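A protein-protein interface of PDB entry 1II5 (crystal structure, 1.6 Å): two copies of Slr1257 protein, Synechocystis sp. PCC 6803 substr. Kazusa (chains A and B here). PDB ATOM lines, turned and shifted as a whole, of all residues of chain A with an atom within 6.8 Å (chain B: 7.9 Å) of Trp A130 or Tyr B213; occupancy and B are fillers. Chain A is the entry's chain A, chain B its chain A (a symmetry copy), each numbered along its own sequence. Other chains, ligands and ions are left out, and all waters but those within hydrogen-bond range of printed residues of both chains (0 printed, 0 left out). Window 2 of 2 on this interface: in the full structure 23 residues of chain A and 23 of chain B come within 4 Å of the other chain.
Among the printed residues, merely in contact across the chains: Pro A77 with Asn B210 (3.1 Å), Glu A188 with Tyr B213 (3.5 Å), Pro A189 with Tyr B213 (3.5 Å), Pro A77 with Leu B209 (3.6 Å), Pro A77 with Tyr B213 (3.7 Å), Trp A130 with Tyr B213 (3.9 Å), Val A75 with Leu B209 (3.9 Å), Thr A76 with Tyr B213 (3.9 Å), Pro A77 with Val B206 (3.9 Å) and Thr A76 with Leu B209 (3.96 Å).
The side-chain hydroxyl (OG) of Ser A74 is in hydrogen-bond range of the side-chain carboxylate (OE1) of Glu A188.
N of Val A75 sits at hydrogen-bond distance from O of Pro A189 (2.9 Å).
The side-chain hydroxyl (OG1) of Thr A126 is in hydrogen-bond range of the side-chain carboxylate (OE1) of Glu A188.
NE1 of Trp A130 sits at hydrogen-bond distance from OE2 of Glu A188 (2.7 Å).
OG of Ser A186 sits close to OE2 of Glu A188, 3.4 Å away.
The backbone carbonyl oxygen of Val B206 lies close to the side-chain amide nitrogen of Asn B210, 3.5 Å away.
No position is printed for both chains.
Of the 11 pairs that touch across the chains among the printed residues, none has its exchanged pair printed and touching as well.
The side-chain hydroxyl of Tyr B213 is in hydrogen-bond range of the backbone carbonyl oxygen of Val A75 (2.6 Å).
Of the 13 printed residues of chain B, 4 touch a printed residue of chain A.
Printed residues of chain B that touch a printed residue of chain A: Val B206, Leu B209, Asn B210 and Tyr B213.
Hydrophobic or aromatic side chains of chain B within 4 Å of the printed part of chain A: Val B206, Leu B209 and Tyr B213.
Of the 25 printed residues of chain A, 6 touch a printed residue of chain B.
Printed residues of chain A that touch a printed residue of chain B: Val A75, Thr A76, Pro A77, Trp A130, Glu A188 and Pro A189.
Hydrophobic or aromatic side chains of chain A within 4 Å of the printed part of chain B: Val A75, Pro A77, Trp A130 and Pro A189.
Among the printed residues, no Asp or Glu carboxylate lies within 4 Å of a Lys or Arg side-chain nitrogen of the other chain.
Of chain B, only Tyr B213 (3.9 Å) comes within 4 Å of Trp A130.
Printed residues of chain A within 4 Å of Tyr B213: Val A75, Thr A76, Pro A77, Trp A130, Glu A188 and Pro A189.
Printed residues of chain B within 4 Å of Pro A77: Val B206 (3.9 Å), Leu B209 (3.6 Å), Asn B210 (3.1 Å) and Tyr B213 (3.7 Å).
Printed residues of chain A within 4 Å of Asn B210: Pro A77 (3.1 Å).
Of the printed residues of chain A, Leu B209 touches Val A75 (3.9 Å), Thr A76 (3.96 Å) and Pro A77 (3.6 Å).
Of the printed residues of chain B, Val A75 touches Leu B209 and Tyr B213.
Leu A187 touches none of the printed residues of chain B.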
ATOM      1  N   SER A  74     -17.129 -17.395 -11.852  1.00  0.00           N
ATOM      2  CA  SER A  74     -17.776 -16.145 -11.465  1.00  0.00           C
ATOM      3  C   SER A  74     -17.515 -15.836  -9.990  1.00  0.00           C
ATOM      4  O   SER A  74     -17.631 -16.715  -9.134  1.00  0.00           O
ATOM      5  CB  SER A  74     -19.281 -16.223 -11.701  1.00  0.00           C
ATOM      6  OG  SER A  74     -19.571 -16.379 -13.078  1.00  0.00           O
ATOM      7  N   VAL A  75     -17.105 -14.598  -9.719  1.00  0.00           N
ATOM      8  CA  VAL A  75     -16.845 -14.141  -8.354  1.00  0.00           C
ATOM      9  C   VAL A  75     -18.190 -13.680  -7.807  1.00  0.00           C
ATOM     10  O   VAL A  75     -18.713 -12.639  -8.213  1.00  0.00           O
ATOM     11  CB  VAL A  75     -15.837 -12.951  -8.318  1.00  0.00           C
ATOM     12  CG1 VAL A  75     -15.497 -12.589  -6.875  1.00  0.00           C
ATOM     13  CG2 VAL A  75     -14.568 -13.294  -9.085  1.00  0.00           C
ATOM     14  N   THR A  76     -18.768 -14.473  -6.910  1.00  0.00           N
ATOM     15  CA  THR A  76     -20.067 -14.151  -6.324  1.00  0.00           C
ATOM     16  C   THR A  76     -19.943 -14.053  -4.807  1.00  0.00           C
ATOM     17  O   THR A  76     -19.008 -14.613  -4.220  1.00  0.00           O
ATOM     18  CB  THR A  76     -21.110 -15.246  -6.631  1.00  0.00           C
ATOM     19  OG1 THR A  76     -20.724 -16.459  -5.974  1.00  0.00           O
ATOM     20  CG2 THR A  76     -21.209 -15.494  -8.127  1.00  0.00           C
ATOM     21  N   PRO A  77     -20.897 -13.355  -4.156  1.00  0.00           N
ATOM     22  CA  PRO A  77     -20.927 -13.170  -2.698  1.00  0.00           C
ATOM     23  C   PRO A  77     -20.951 -14.515  -1.956  1.00  0.00           C
ATOM     24  O   PRO A  77     -20.237 -14.704  -0.969  1.00  0.00           O
ATOM     25  CB  PRO A  77     -22.239 -12.416  -2.481  1.00  0.00           C
ATOM     26  CG  PRO A  77     -22.411 -11.646  -3.745  1.00  0.00           C
ATOM     27  CD  PRO A  77     -22.014 -12.634  -4.797  1.00  0.00           C
ATOM     28  N   ILE A  96     -24.030 -13.166 -18.392  1.00  0.00           N
ATOM     29  CA  ILE A  96     -24.819 -14.382 -18.436  1.00  0.00           C
ATOM     30  C   ILE A  96     -25.913 -14.084 -19.467  1.00  0.00           C
ATOM     31  O   ILE A  96     -26.593 -13.068 -19.373  1.00  0.00           O
ATOM     32  CB  ILE A  96     -25.410 -14.702 -17.043  1.00  0.00           C
ATOM     33  CG1 ILE A  96     -24.280 -14.815 -16.014  1.00  0.00           C
ATOM     34  CG2 ILE A  96     -26.227 -15.985 -17.073  1.00  0.00           C
ATOM     35  CD1 ILE A  96     -23.131 -15.728 -16.422  1.00  0.00           C
ATOM     36  N   LEU A 114     -38.513 -13.716 -18.825  1.00  0.00           N
ATOM     37  CA  LEU A 114     -38.065 -15.025 -18.356  1.00  0.00           C
ATOM     38  C   LEU A 114     -39.085 -15.708 -17.446  1.00  0.00           C
ATOM     39  O   LEU A 114     -39.115 -16.936 -17.353  1.00  0.00           O
ATOM     40  CB  LEU A 114     -36.732 -14.894 -17.618  1.00  0.00           C
ATOM     41  CG  LEU A 114     -35.497 -14.680 -18.486  1.00  0.00           C
ATOM     42  CD1 LEU A 114     -34.299 -14.324 -17.610  1.00  0.00           C
ATOM     43  CD2 LEU A 114     -35.233 -15.940 -19.297  1.00  0.00           C
ATOM     44  N   THR A 125     -23.907 -23.670 -11.693  1.00  0.00           N
ATOM     45  CA  THR A 125     -23.413 -22.485 -12.385  1.00  0.00           C
ATOM     46  C   THR A 125     -24.276 -21.366 -11.842  1.00  0.00           C
ATOM     47  O   THR A 125     -25.351 -21.617 -11.288  1.00  0.00           O
ATOM     48  CB  THR A 125     -23.535 -22.570 -13.929  1.00  0.00           C
ATOM     49  OG1 THR A 125     -24.907 -22.733 -14.298  1.00  0.00           O
ATOM     50  CG2 THR A 125     -22.704 -23.729 -14.470  1.00  0.00           C
ATOM     51  N   THR A 126     -23.793 -20.137 -11.954  1.00  0.00           N
ATOM     52  CA  THR A 126     -24.538 -18.997 -11.450  1.00  0.00           C
ATOM     53  C   THR A 126     -25.892 -18.861 -12.144  1.00  0.00           C
ATOM     54  O   THR A 126     -26.831 -18.311 -11.572  1.00  0.00           O
ATOM     55  CB  THR A 126     -23.731 -17.696 -11.605  1.00  0.00           C
ATOM     56  OG1 THR A 126     -23.370 -17.523 -12.979  1.00  0.00           O
ATOM     57  CG2 THR A 126     -22.467 -17.744 -10.751  1.00  0.00           C
ATOM     58  N   ALA A 127     -25.996 -19.405 -13.358  1.00  0.00           N
ATOM     59  CA  ALA A 127     -27.243 -19.355 -14.129  1.00  0.00           C
ATOM     60  C   ALA A 127     -28.410 -20.006 -13.386  1.00  0.00           C
ATOM     61  O   ALA A 127     -29.556 -19.580 -13.534  1.00  0.00           O
ATOM     62  CB  ALA A 127     -27.055 -20.009 -15.495  1.00  0.00           C
ATOM     63  N   VAL A 128     -28.126 -21.033 -12.586  1.00  0.00           N
ATOM     64  CA  VAL A 128     -29.178 -21.703 -11.827  1.00  0.00           C
ATOM     65  C   VAL A 128     -29.870 -20.702 -10.900  1.00  0.00           C
ATOM     66  O   VAL A 128     -31.101 -20.610 -10.869  1.00  0.00           O
ATOM     67  CB  VAL A 128     -28.621 -22.878 -10.984  1.00  0.00           C
ATOM     68  CG1 VAL A 128     -29.743 -23.534 -10.191  1.00  0.00           C
ATOM     69  CG2 VAL A 128     -27.942 -23.900 -11.883  1.00  0.00           C
ATOM     70  N   ASP A 129     -29.061 -19.905 -10.204  1.00  0.00           N
ATOM     71  CA  ASP A 129     -29.572 -18.906  -9.270  1.00  0.00           C
ATOM     72  C   ASP A 129     -30.269 -17.737  -9.963  1.00  0.00           C
ATOM     73  O   ASP A 129     -31.280 -17.243  -9.472  1.00  0.00           O
ATOM     74  CB  ASP A 129     -28.446 -18.411  -8.359  1.00  0.00           C
ATOM     75  CG  ASP A 129     -27.785 -19.548  -7.584  1.00  0.00           C
ATOM     76  OD1 ASP A 129     -28.505 -20.476  -7.155  1.00  0.00           O
ATOM     77  OD2 ASP A 129     -26.548 -19.525  -7.413  1.00  0.00           O
ATOM     78  N   TRP A 130     -29.735 -17.299 -11.101  1.00  0.00           N
ATOM     79  CA  TRP A 130     -30.349 -16.199 -11.840  1.00  0.00           C
ATOM     80  C   TRP A 130     -31.697 -16.610 -12.437  1.00  0.00           C
ATOM     81  O   TRP A 130     -32.639 -15.817 -12.452  1.00  0.00           O
ATOM     82  CB  TRP A 130     -29.419 -15.698 -12.949  1.00  0.00           C
ATOM     83  CG  TRP A 130     -28.325 -14.819 -12.445  1.00  0.00           C
ATOM     84  CD1 TRP A 130     -26.987 -15.072 -12.487  1.00  0.00           C
ATOM     85  CD2 TRP A 130     -28.478 -13.545 -11.808  1.00  0.00           C
ATOM     86  NE1 TRP A 130     -26.296 -14.035 -11.912  1.00  0.00           N
ATOM     87  CE2 TRP A 130     -27.182 -13.082 -11.488  1.00  0.00           C
ATOM     88  CE3 TRP A 130     -29.580 -12.744 -11.478  1.00  0.00           C
ATOM     89  CZ2 TRP A 130     -26.957 -11.853 -10.847  1.00  0.00           C
ATOM     90  CZ3 TRP A 130     -29.359 -11.524 -10.845  1.00  0.00           C
ATOM     91  CH2 TRP A 130     -28.056 -11.093 -10.535  1.00  0.00           C
ATOM     92  N   ALA A 131     -31.779 -17.853 -12.916  1.00  0.00           N
ATOM     93  CA  ALA A 131     -33.011 -18.382 -13.508  1.00  0.00           C
ATOM     94  C   ALA A 131     -34.083 -18.481 -12.434  1.00  0.00           C
ATOM     95  O   ALA A 131     -35.247 -18.190 -12.688  1.00  0.00           O
ATOM     96  CB  ALA A 131     -32.768 -19.738 -14.136  1.00  0.00           C
ATOM     97  N   ASN A 132     -33.682 -18.884 -11.231  1.00  0.00           N
ATOM     98  CA  ASN A 132     -34.615 -18.985 -10.112  1.00  0.00           C
ATOM     99  C   ASN A 132     -35.047 -17.582  -9.673  1.00  0.00           C
ATOM    100  O   ASN A 132     -36.227 -17.346  -9.398  1.00  0.00           O
ATOM    101  CB  ASN A 132     -33.975 -19.734  -8.932  1.00  0.00           C
ATOM    102  CG  ASN A 132     -33.761 -21.209  -9.219  1.00  0.00           C
ATOM    103  OD1 ASN A 132     -34.547 -21.832  -9.930  1.00  0.00           O
ATOM    104  ND2 ASN A 132     -32.693 -21.778  -8.668  1.00  0.00           N
ATOM    105  N   PHE A 133     -34.094 -16.651  -9.638  1.00  0.00           N
ATOM    106  CA  PHE A 133     -34.373 -15.272  -9.241  1.00  0.00           C
ATOM    107  C   PHE A 133     -35.366 -14.589 -10.185  1.00  0.00           C
ATOM    108  O   PHE A 133     -36.206 -13.806  -9.741  1.00  0.00           O
ATOM    109  CB  PHE A 133     -33.078 -14.452  -9.167  1.00  0.00           C
ATOM    110  CG  PHE A 133     -33.298 -12.994  -8.857  1.00  0.00           C
ATOM    111  CD1 PHE A 133     -33.563 -12.576  -7.557  1.00  0.00           C
ATOM    112  CD2 PHE A 133     -33.258 -12.039  -9.870  1.00  0.00           C
ATOM    113  CE1 PHE A 133     -33.793 -11.229  -7.269  1.00  0.00           C
ATOM    114  CE2 PHE A 133     -33.487 -10.691  -9.594  1.00  0.00           C
ATOM    115  CZ  PHE A 133     -33.753 -10.285  -8.290  1.00  0.00           C
ATOM    116  N   TYR A 134     -35.259 -14.882 -11.479  1.00  0.00           N
ATOM    117  CA  TYR A 134     -36.160 -14.294 -12.467  1.00  0.00           C
ATOM    118  C   TYR A 134     -37.450 -15.085 -12.680  1.00  0.00           C
ATOM    119  O   TYR A 134     -38.210 -14.828 -13.612  1.00  0.00           O
ATOM    120  CB  TYR A 134     -35.418 -14.015 -13.772  1.00  0.00           C
ATOM    121  CG  TYR A 134     -34.580 -12.766 -13.651  1.00  0.00           C
ATOM    122  CD1 TYR A 134     -33.190 -12.809 -13.780  1.00  0.00           C
ATOM    123  CD2 TYR A 134     -35.179 -11.544 -13.335  1.00  0.00           C
ATOM    124  CE1 TYR A 134     -32.421 -11.663 -13.590  1.00  0.00           C
ATOM    125  CE2 TYR A 134     -34.424 -10.399 -13.142  1.00  0.00           C
ATOM    126  CZ  TYR A 134     -33.048 -10.464 -13.269  1.00  0.00           C
ATOM    127  OH  TYR A 134     -32.302  -9.328 -13.069  1.00  0.00           O
ATOM    128  N   GLN A 135     -37.687 -16.036 -11.777  1.00  0.00           N
ATOM    129  CA  GLN A 135     -38.883 -16.873 -11.769  1.00  0.00           C
ATOM    130  C   GLN A 135     -39.178 -17.732 -12.987  1.00  0.00           C
ATOM    131  O   GLN A 135     -40.341 -17.956 -13.333  1.00  0.00           O
ATOM    132  CB  GLN A 135     -40.105 -16.033 -11.415  1.00  0.00           C
ATOM    133  CG  GLN A 135     -40.065 -15.460 -10.012  1.00  0.00           C
ATOM    134  CD  GLN A 135     -41.174 -14.464  -9.775  1.00  0.00           C
ATOM    135  OE1 GLN A 135     -42.115 -14.367 -10.562  1.00  0.00           O
ATOM    136  NE2 GLN A 135     -41.072 -13.713  -8.689  1.00  0.00           N
ATOM    137  N   ALA A 136     -38.126 -18.224 -13.630  1.00  0.00           N
ATOM    138  CA  ALA A 136     -38.284 -19.097 -14.783  1.00  0.00           C
ATOM    139  C   ALA A 136     -38.614 -20.512 -14.296  1.00  0.00           C
ATOM    140  O   ALA A 136     -38.551 -20.799 -13.095  1.00  0.00           O
ATOM    141  CB  ALA A 136     -37.000 -19.112 -15.612  1.00  0.00           C
ATOM    142  N   VAL A 138     -37.147 -23.475 -14.156  1.00  0.00           N
ATOM    143  CA  VAL A 138     -35.812 -24.051 -14.259  1.00  0.00           C
ATOM    144  C   VAL A 138     -35.690 -25.555 -14.409  1.00  0.00           C
ATOM    145  O   VAL A 138     -36.189 -26.315 -13.590  1.00  0.00           O
ATOM    146  CB  VAL A 138     -34.964 -23.609 -13.064  1.00  0.00           C
ATOM    147  CG1 VAL A 138     -33.524 -24.057 -13.247  1.00  0.00           C
ATOM    148  CG2 VAL A 138     -35.052 -22.104 -12.903  1.00  0.00           C
ATOM    149  N   MET A 160     -29.956 -20.749 -20.385  1.00  0.00           N
ATOM    150  CA  MET A 160     -29.279 -19.632 -19.728  1.00  0.00           C
ATOM    151  C   MET A 160     -27.887 -20.103 -19.335  1.00  0.00           C
ATOM    152  O   MET A 160     -27.742 -21.108 -18.640  1.00  0.00           O
ATOM    153  CB  MET A 160     -30.046 -19.179 -18.489  1.00  0.00           C
ATOM    154  CG  MET A 160     -29.546 -17.864 -17.931  1.00  0.00           C
ATOM    155  SD  MET A 160     -30.303 -17.439 -16.354  1.00  0.00           S
ATOM    156  CE  MET A 160     -31.913 -16.812 -16.897  1.00  0.00           C
ATOM    157  N   VAL A 185     -28.556 -11.120 -18.562  1.00  0.00           N
ATOM    158  CA  VAL A 185     -29.180 -11.410 -17.280  1.00  0.00           C
ATOM    159  C   VAL A 185     -28.336 -10.862 -16.132  1.00  0.00           C
ATOM    160  O   VAL A 185     -28.864 -10.497 -15.078  1.00  0.00           O
ATOM    161  CB  VAL A 185     -29.390 -12.925 -17.098  1.00  0.00           C
ATOM    162  CG1 VAL A 185     -30.022 -13.211 -15.760  1.00  0.00           C
ATOM    163  CG2 VAL A 185     -30.270 -13.470 -18.204  1.00  0.00           C
ATOM    164  N   SER A 186     -27.026 -10.785 -16.360  1.00  0.00           N
ATOM    165  CA  SER A 186     -26.090 -10.282 -15.367  1.00  0.00           C
ATOM    166  C   SER A 186     -24.708 -10.056 -15.956  1.00  0.00           C
ATOM    167  O   SER A 186     -24.402 -10.529 -17.049  1.00  0.00           O
ATOM    168  CB  SER A 186     -25.970 -11.294 -14.227  1.00  0.00           C
ATOM    169  OG  SER A 186     -24.822 -11.042 -13.429  1.00  0.00           O
ATOM    170  N   LEU A 187     -23.889  -9.309 -15.220  1.00  0.00           N
ATOM    171  CA  LEU A 187     -22.504  -9.043 -15.588  1.00  0.00           C
ATOM    172  C   LEU A 187     -21.739  -9.613 -14.410  1.00  0.00           C
ATOM    173  O   LEU A 187     -22.010  -9.247 -13.266  1.00  0.00           O
ATOM    174  CB  LEU A 187     -22.227  -7.548 -15.695  1.00  0.00           C
ATOM    175  CG  LEU A 187     -21.899  -7.044 -17.094  1.00  0.00           C
ATOM    176  CD1 LEU A 187     -23.176  -6.609 -17.792  1.00  0.00           C
ATOM    177  CD2 LEU A 187     -20.913  -5.889 -17.001  1.00  0.00           C
ATOM    178  N   GLU A 188     -20.827 -10.538 -14.681  1.00  0.00           N
ATOM    179  CA  GLU A 188     -20.058 -11.181 -13.627  1.00  0.00           C
ATOM    180  C   GLU A 188     -18.590 -11.264 -13.961  1.00  0.00           C
ATOM    181  O   GLU A 188     -18.224 -11.577 -15.088  1.00  0.00           O
ATOM    182  CB  GLU A 188     -20.560 -12.611 -13.421  1.00  0.00           C
ATOM    183  CG  GLU A 188     -21.993 -12.692 -12.978  1.00  0.00           C
ATOM    184  CD  GLU A 188     -22.561 -14.098 -12.970  1.00  0.00           C
ATOM    185  OE1 GLU A 188     -21.840 -15.086 -13.241  1.00  0.00           O
ATOM    186  OE2 GLU A 188     -23.764 -14.208 -12.698  1.00  0.00           O
ATOM    187  N   PRO A 189     -17.720 -10.991 -12.979  1.00  0.00           N
ATOM    188  CA  PRO A 189     -16.279 -11.062 -13.208  1.00  0.00           C
ATOM    189  C   PRO A 189     -15.797 -12.509 -12.984  1.00  0.00           C
ATOM    190  O   PRO A 189     -16.395 -13.241 -12.198  1.00  0.00           O
ATOM    191  CB  PRO A 189     -15.733 -10.117 -12.140  1.00  0.00           C
ATOM    192  CG  PRO A 189     -16.662 -10.320 -11.005  1.00  0.00           C
ATOM    193  CD  PRO A 189     -18.024 -10.412 -11.656  1.00  0.00           C
ATOM    194  N   VAL B 206     -17.208 -10.016   0.752  1.00  0.00           N
ATOM    195  CA  VAL B 206     -18.563 -10.534   0.657  1.00  0.00           C
ATOM    196  C   VAL B 206     -19.585  -9.400   0.610  1.00  0.00           C
ATOM    197  O   VAL B 206     -20.463  -9.389  -0.257  1.00  0.00           O
ATOM    198  CB  VAL B 206     -18.870 -11.519   1.808  1.00  0.00           C
ATOM    199  CG1 VAL B 206     -20.346 -11.912   1.813  1.00  0.00           C
ATOM    200  CG2 VAL B 206     -17.991 -12.756   1.658  1.00  0.00           C
ATOM    201  N   GLU B 207     -19.429  -8.415   1.493  1.00  0.00           N
ATOM    202  CA  GLU B 207     -20.356  -7.286   1.527  1.00  0.00           C
ATOM    203  C   GLU B 207     -20.285  -6.389   0.300  1.00  0.00           C
ATOM    204  O   GLU B 207     -21.310  -5.936  -0.190  1.00  0.00           O
ATOM    205  CB  GLU B 207     -20.185  -6.454   2.802  1.00  0.00           C
ATOM    206  CG  GLU B 207     -20.886  -7.057   4.014  1.00  0.00           C
ATOM    207  CD  GLU B 207     -22.366  -7.399   3.758  1.00  0.00           C
ATOM    208  OE1 GLU B 207     -22.885  -8.301   4.448  1.00  0.00           O
ATOM    209  OE2 GLU B 207     -23.012  -6.775   2.885  1.00  0.00           O
ATOM    210  N   MET B 208     -19.084  -6.149  -0.208  1.00  0.00           N
ATOM    211  CA  MET B 208     -18.930  -5.316  -1.393  1.00  0.00           C
ATOM    212  C   MET B 208     -19.549  -6.034  -2.599  1.00  0.00           C
ATOM    213  O   MET B 208     -20.205  -5.407  -3.434  1.00  0.00           O
ATOM    214  CB  MET B 208     -17.451  -4.999  -1.632  1.00  0.00           C
ATOM    215  CG  MET B 208     -16.905  -3.936  -0.678  1.00  0.00           C
ATOM    216  SD  MET B 208     -15.123  -3.699  -0.810  1.00  0.00           S
ATOM    217  CE  MET B 208     -15.004  -2.811  -2.393  1.00  0.00           C
ATOM    218  N   LEU B 209     -19.390  -7.357  -2.648  1.00  0.00           N
ATOM    219  CA  LEU B 209     -19.956  -8.151  -3.734  1.00  0.00           C
ATOM    220  C   LEU B 209     -21.491  -8.141  -3.664  1.00  0.00           C
ATOM    221  O   LEU B 209     -22.156  -8.075  -4.695  1.00  0.00           O
ATOM    222  CB  LEU B 209     -19.390  -9.577  -3.717  1.00  0.00           C
ATOM    223  CG  LEU B 209     -17.933  -9.694  -4.200  1.00  0.00           C
ATOM    224  CD1 LEU B 209     -17.328 -11.043  -3.840  1.00  0.00           C
ATOM    225  CD2 LEU B 209     -17.865  -9.461  -5.703  1.00  0.00           C
ATOM    226  N   ASN B 210     -22.042  -8.171  -2.447  1.00  0.00           N
ATOM    227  CA  ASN B 210     -23.495  -8.123  -2.241  1.00  0.00           C
ATOM    228  C   ASN B 210     -24.031  -6.802  -2.771  1.00  0.00           C
ATOM    229  O   ASN B 210     -25.049  -6.768  -3.455  1.00  0.00           O
ATOM    230  CB  ASN B 210     -23.837  -8.201  -0.750  1.00  0.00           C
ATOM    231  CG  ASN B 210     -23.909  -9.613  -0.241  1.00  0.00           C
ATOM    232  OD1 ASN B 210     -24.201 -10.539  -0.993  1.00  0.00           O
ATOM    233  ND2 ASN B 210     -23.668  -9.788   1.053  1.00  0.00           N
ATOM    234  N   LEU B 211     -23.352  -5.713  -2.406  1.00  0.00           N
ATOM    235  CA  LEU B 211     -23.730  -4.368  -2.833  1.00  0.00           C
ATOM    236  C   LEU B 211     -23.655  -4.245  -4.352  1.00  0.00           C
ATOM    237  O   LEU B 211     -24.501  -3.607  -4.975  1.00  0.00           O
ATOM    238  CB  LEU B 211     -22.808  -3.327  -2.176  1.00  0.00           C
ATOM    239  CG  LEU B 211     -22.959  -3.154  -0.661  1.00  0.00           C
ATOM    240  CD1 LEU B 211     -21.846  -2.277  -0.107  1.00  0.00           C
ATOM    241  CD2 LEU B 211     -24.318  -2.556  -0.351  1.00  0.00           C
ATOM    242  N   LEU B 212     -22.644  -4.886  -4.934  1.00  0.00           N
ATOM    243  CA  LEU B 212     -22.424  -4.872  -6.374  1.00  0.00           C
ATOM    244  C   LEU B 212     -23.537  -5.603  -7.118  1.00  0.00           C
ATOM    245  O   LEU B 212     -24.202  -5.015  -7.962  1.00  0.00           O
ATOM    246  CB  LEU B 212     -21.080  -5.522  -6.691  1.00  0.00           C
ATOM    247  CG  LEU B 212     -20.548  -5.354  -8.106  1.00  0.00           C
ATOM    248  CD1 LEU B 212     -20.362  -3.868  -8.427  1.00  0.00           C
ATOM    249  CD2 LEU B 212     -19.229  -6.113  -8.231  1.00  0.00           C
ATOM    250  N   TYR B 213     -23.753  -6.869  -6.770  1.00  0.00           N
ATOM    251  CA  TYR B 213     -24.777  -7.708  -7.405  1.00  0.00           C
ATOM    252  C   TYR B 213     -26.221  -7.267  -7.178  1.00  0.00           C
ATOM    253  O   TYR B 213     -27.084  -7.514  -8.020  1.00  0.00           O
ATOM    254  CB  TYR B 213     -24.610  -9.170  -6.985  1.00  0.00           C
ATOM    255  CG  TYR B 213     -23.539  -9.909  -7.758  1.00  0.00           C
ATOM    256  CD1 TYR B 213     -22.208  -9.897  -7.338  1.00  0.00           C
ATOM    257  CD2 TYR B 213     -23.862 -10.640  -8.902  1.00  0.00           C
ATOM    258  CE1 TYR B 213     -21.226 -10.602  -8.040  1.00  0.00           C
ATOM    259  CE2 TYR B 213     -22.891 -11.343  -9.608  1.00  0.00           C
ATOM    260  CZ  TYR B 213     -21.577 -11.324  -9.176  1.00  0.00           C
ATOM    261  OH  TYR B 213     -20.623 -12.023  -9.882  1.00  0.00           O
ATOM    262  N   SER B 214     -26.487  -6.617  -6.046  1.00  0.00           N
ATOM    263  CA  SER B 214     -27.834  -6.141  -5.750  1.00  0.00           C
ATOM    264  C   SER B 214     -28.091  -4.792  -6.421  1.00  0.00           C
ATOM    265  O   SER B 214     -29.159  -4.205  -6.251  1.00  0.00           O
ATOM    266  CB  SER B 214     -28.032  -6.027  -4.242  1.00  0.00           C
ATOM    267  OG  SER B 214     -27.081  -5.144  -3.682  1.00  0.00           O
ATOM    268  N   ARG B 215     -27.101  -4.310  -7.174  1.00  0.00           N
ATOM    269  CA  ARG B 215     -27.166  -3.039  -7.899  1.00  0.00           C
ATOM    270  C   ARG B 215     -27.168  -1.803  -6.995  1.00  0.00           C
ATOM    271  O   ARG B 215     -27.447  -0.692  -7.447  1.00  0.00           O
ATOM    272  CB  ARG B 215     -28.375  -3.019  -8.865  1.00  0.00           C
ATOM    273  N   VAL B 216     -26.822  -1.995  -5.724  1.00  0.00           N
ATOM    274  CA  VAL B 216     -26.775  -0.889  -4.772  1.00  0.00           C
ATOM    275  C   VAL B 216     -25.657   0.099  -5.125  1.00  0.00           C
ATOM    276  O   VAL B 216     -25.846   1.319  -5.032  1.00  0.00           O
ATOM    277  CB  VAL B 216     -26.626  -1.402  -3.326  1.00  0.00           C
ATOM    278  CG1 VAL B 216     -26.345  -0.251  -2.374  1.00  0.00           C
ATOM    279  CG2 VAL B 216     -27.901  -2.113  -2.901  1.00  0.00           C
ATOM    280  N   ILE B 217     -24.510  -0.424  -5.560  1.00  0.00           N
ATOM    281  CA  ILE B 217     -23.398   0.438  -5.947  1.00  0.00           C
ATOM    282  C   ILE B 217     -23.796   1.276  -7.167  1.00  0.00           C
ATOM    283  O   ILE B 217     -23.450   2.464  -7.256  1.00  0.00           O
ATOM    284  CB  ILE B 217     -22.113  -0.371  -6.227  1.00  0.00           C
ATOM    285  CG1 ILE B 217     -21.705  -1.145  -4.966  1.00  0.00           C
ATOM    286  CG2 ILE B 217     -20.986   0.556  -6.642  1.00  0.00           C
ATOM    287  CD1 ILE B 217     -20.352  -1.798  -5.048  1.00  0.00           C
ATOM    288  N   ALA B 218     -24.570   0.671  -8.072  1.00  0.00           N
ATOM    289  CA  ALA B 218     -25.043   1.371  -9.266  1.00  0.00           C
ATOM    290  C   ALA B 218     -25.954   2.525  -8.839  1.00  0.00           C
ATOM    291  O   ALA B 218     -25.890   3.615  -9.410  1.00  0.00           O
ATOM    292  CB  ALA B 218     -25.790   0.414 -10.189  1.00  0.00           C
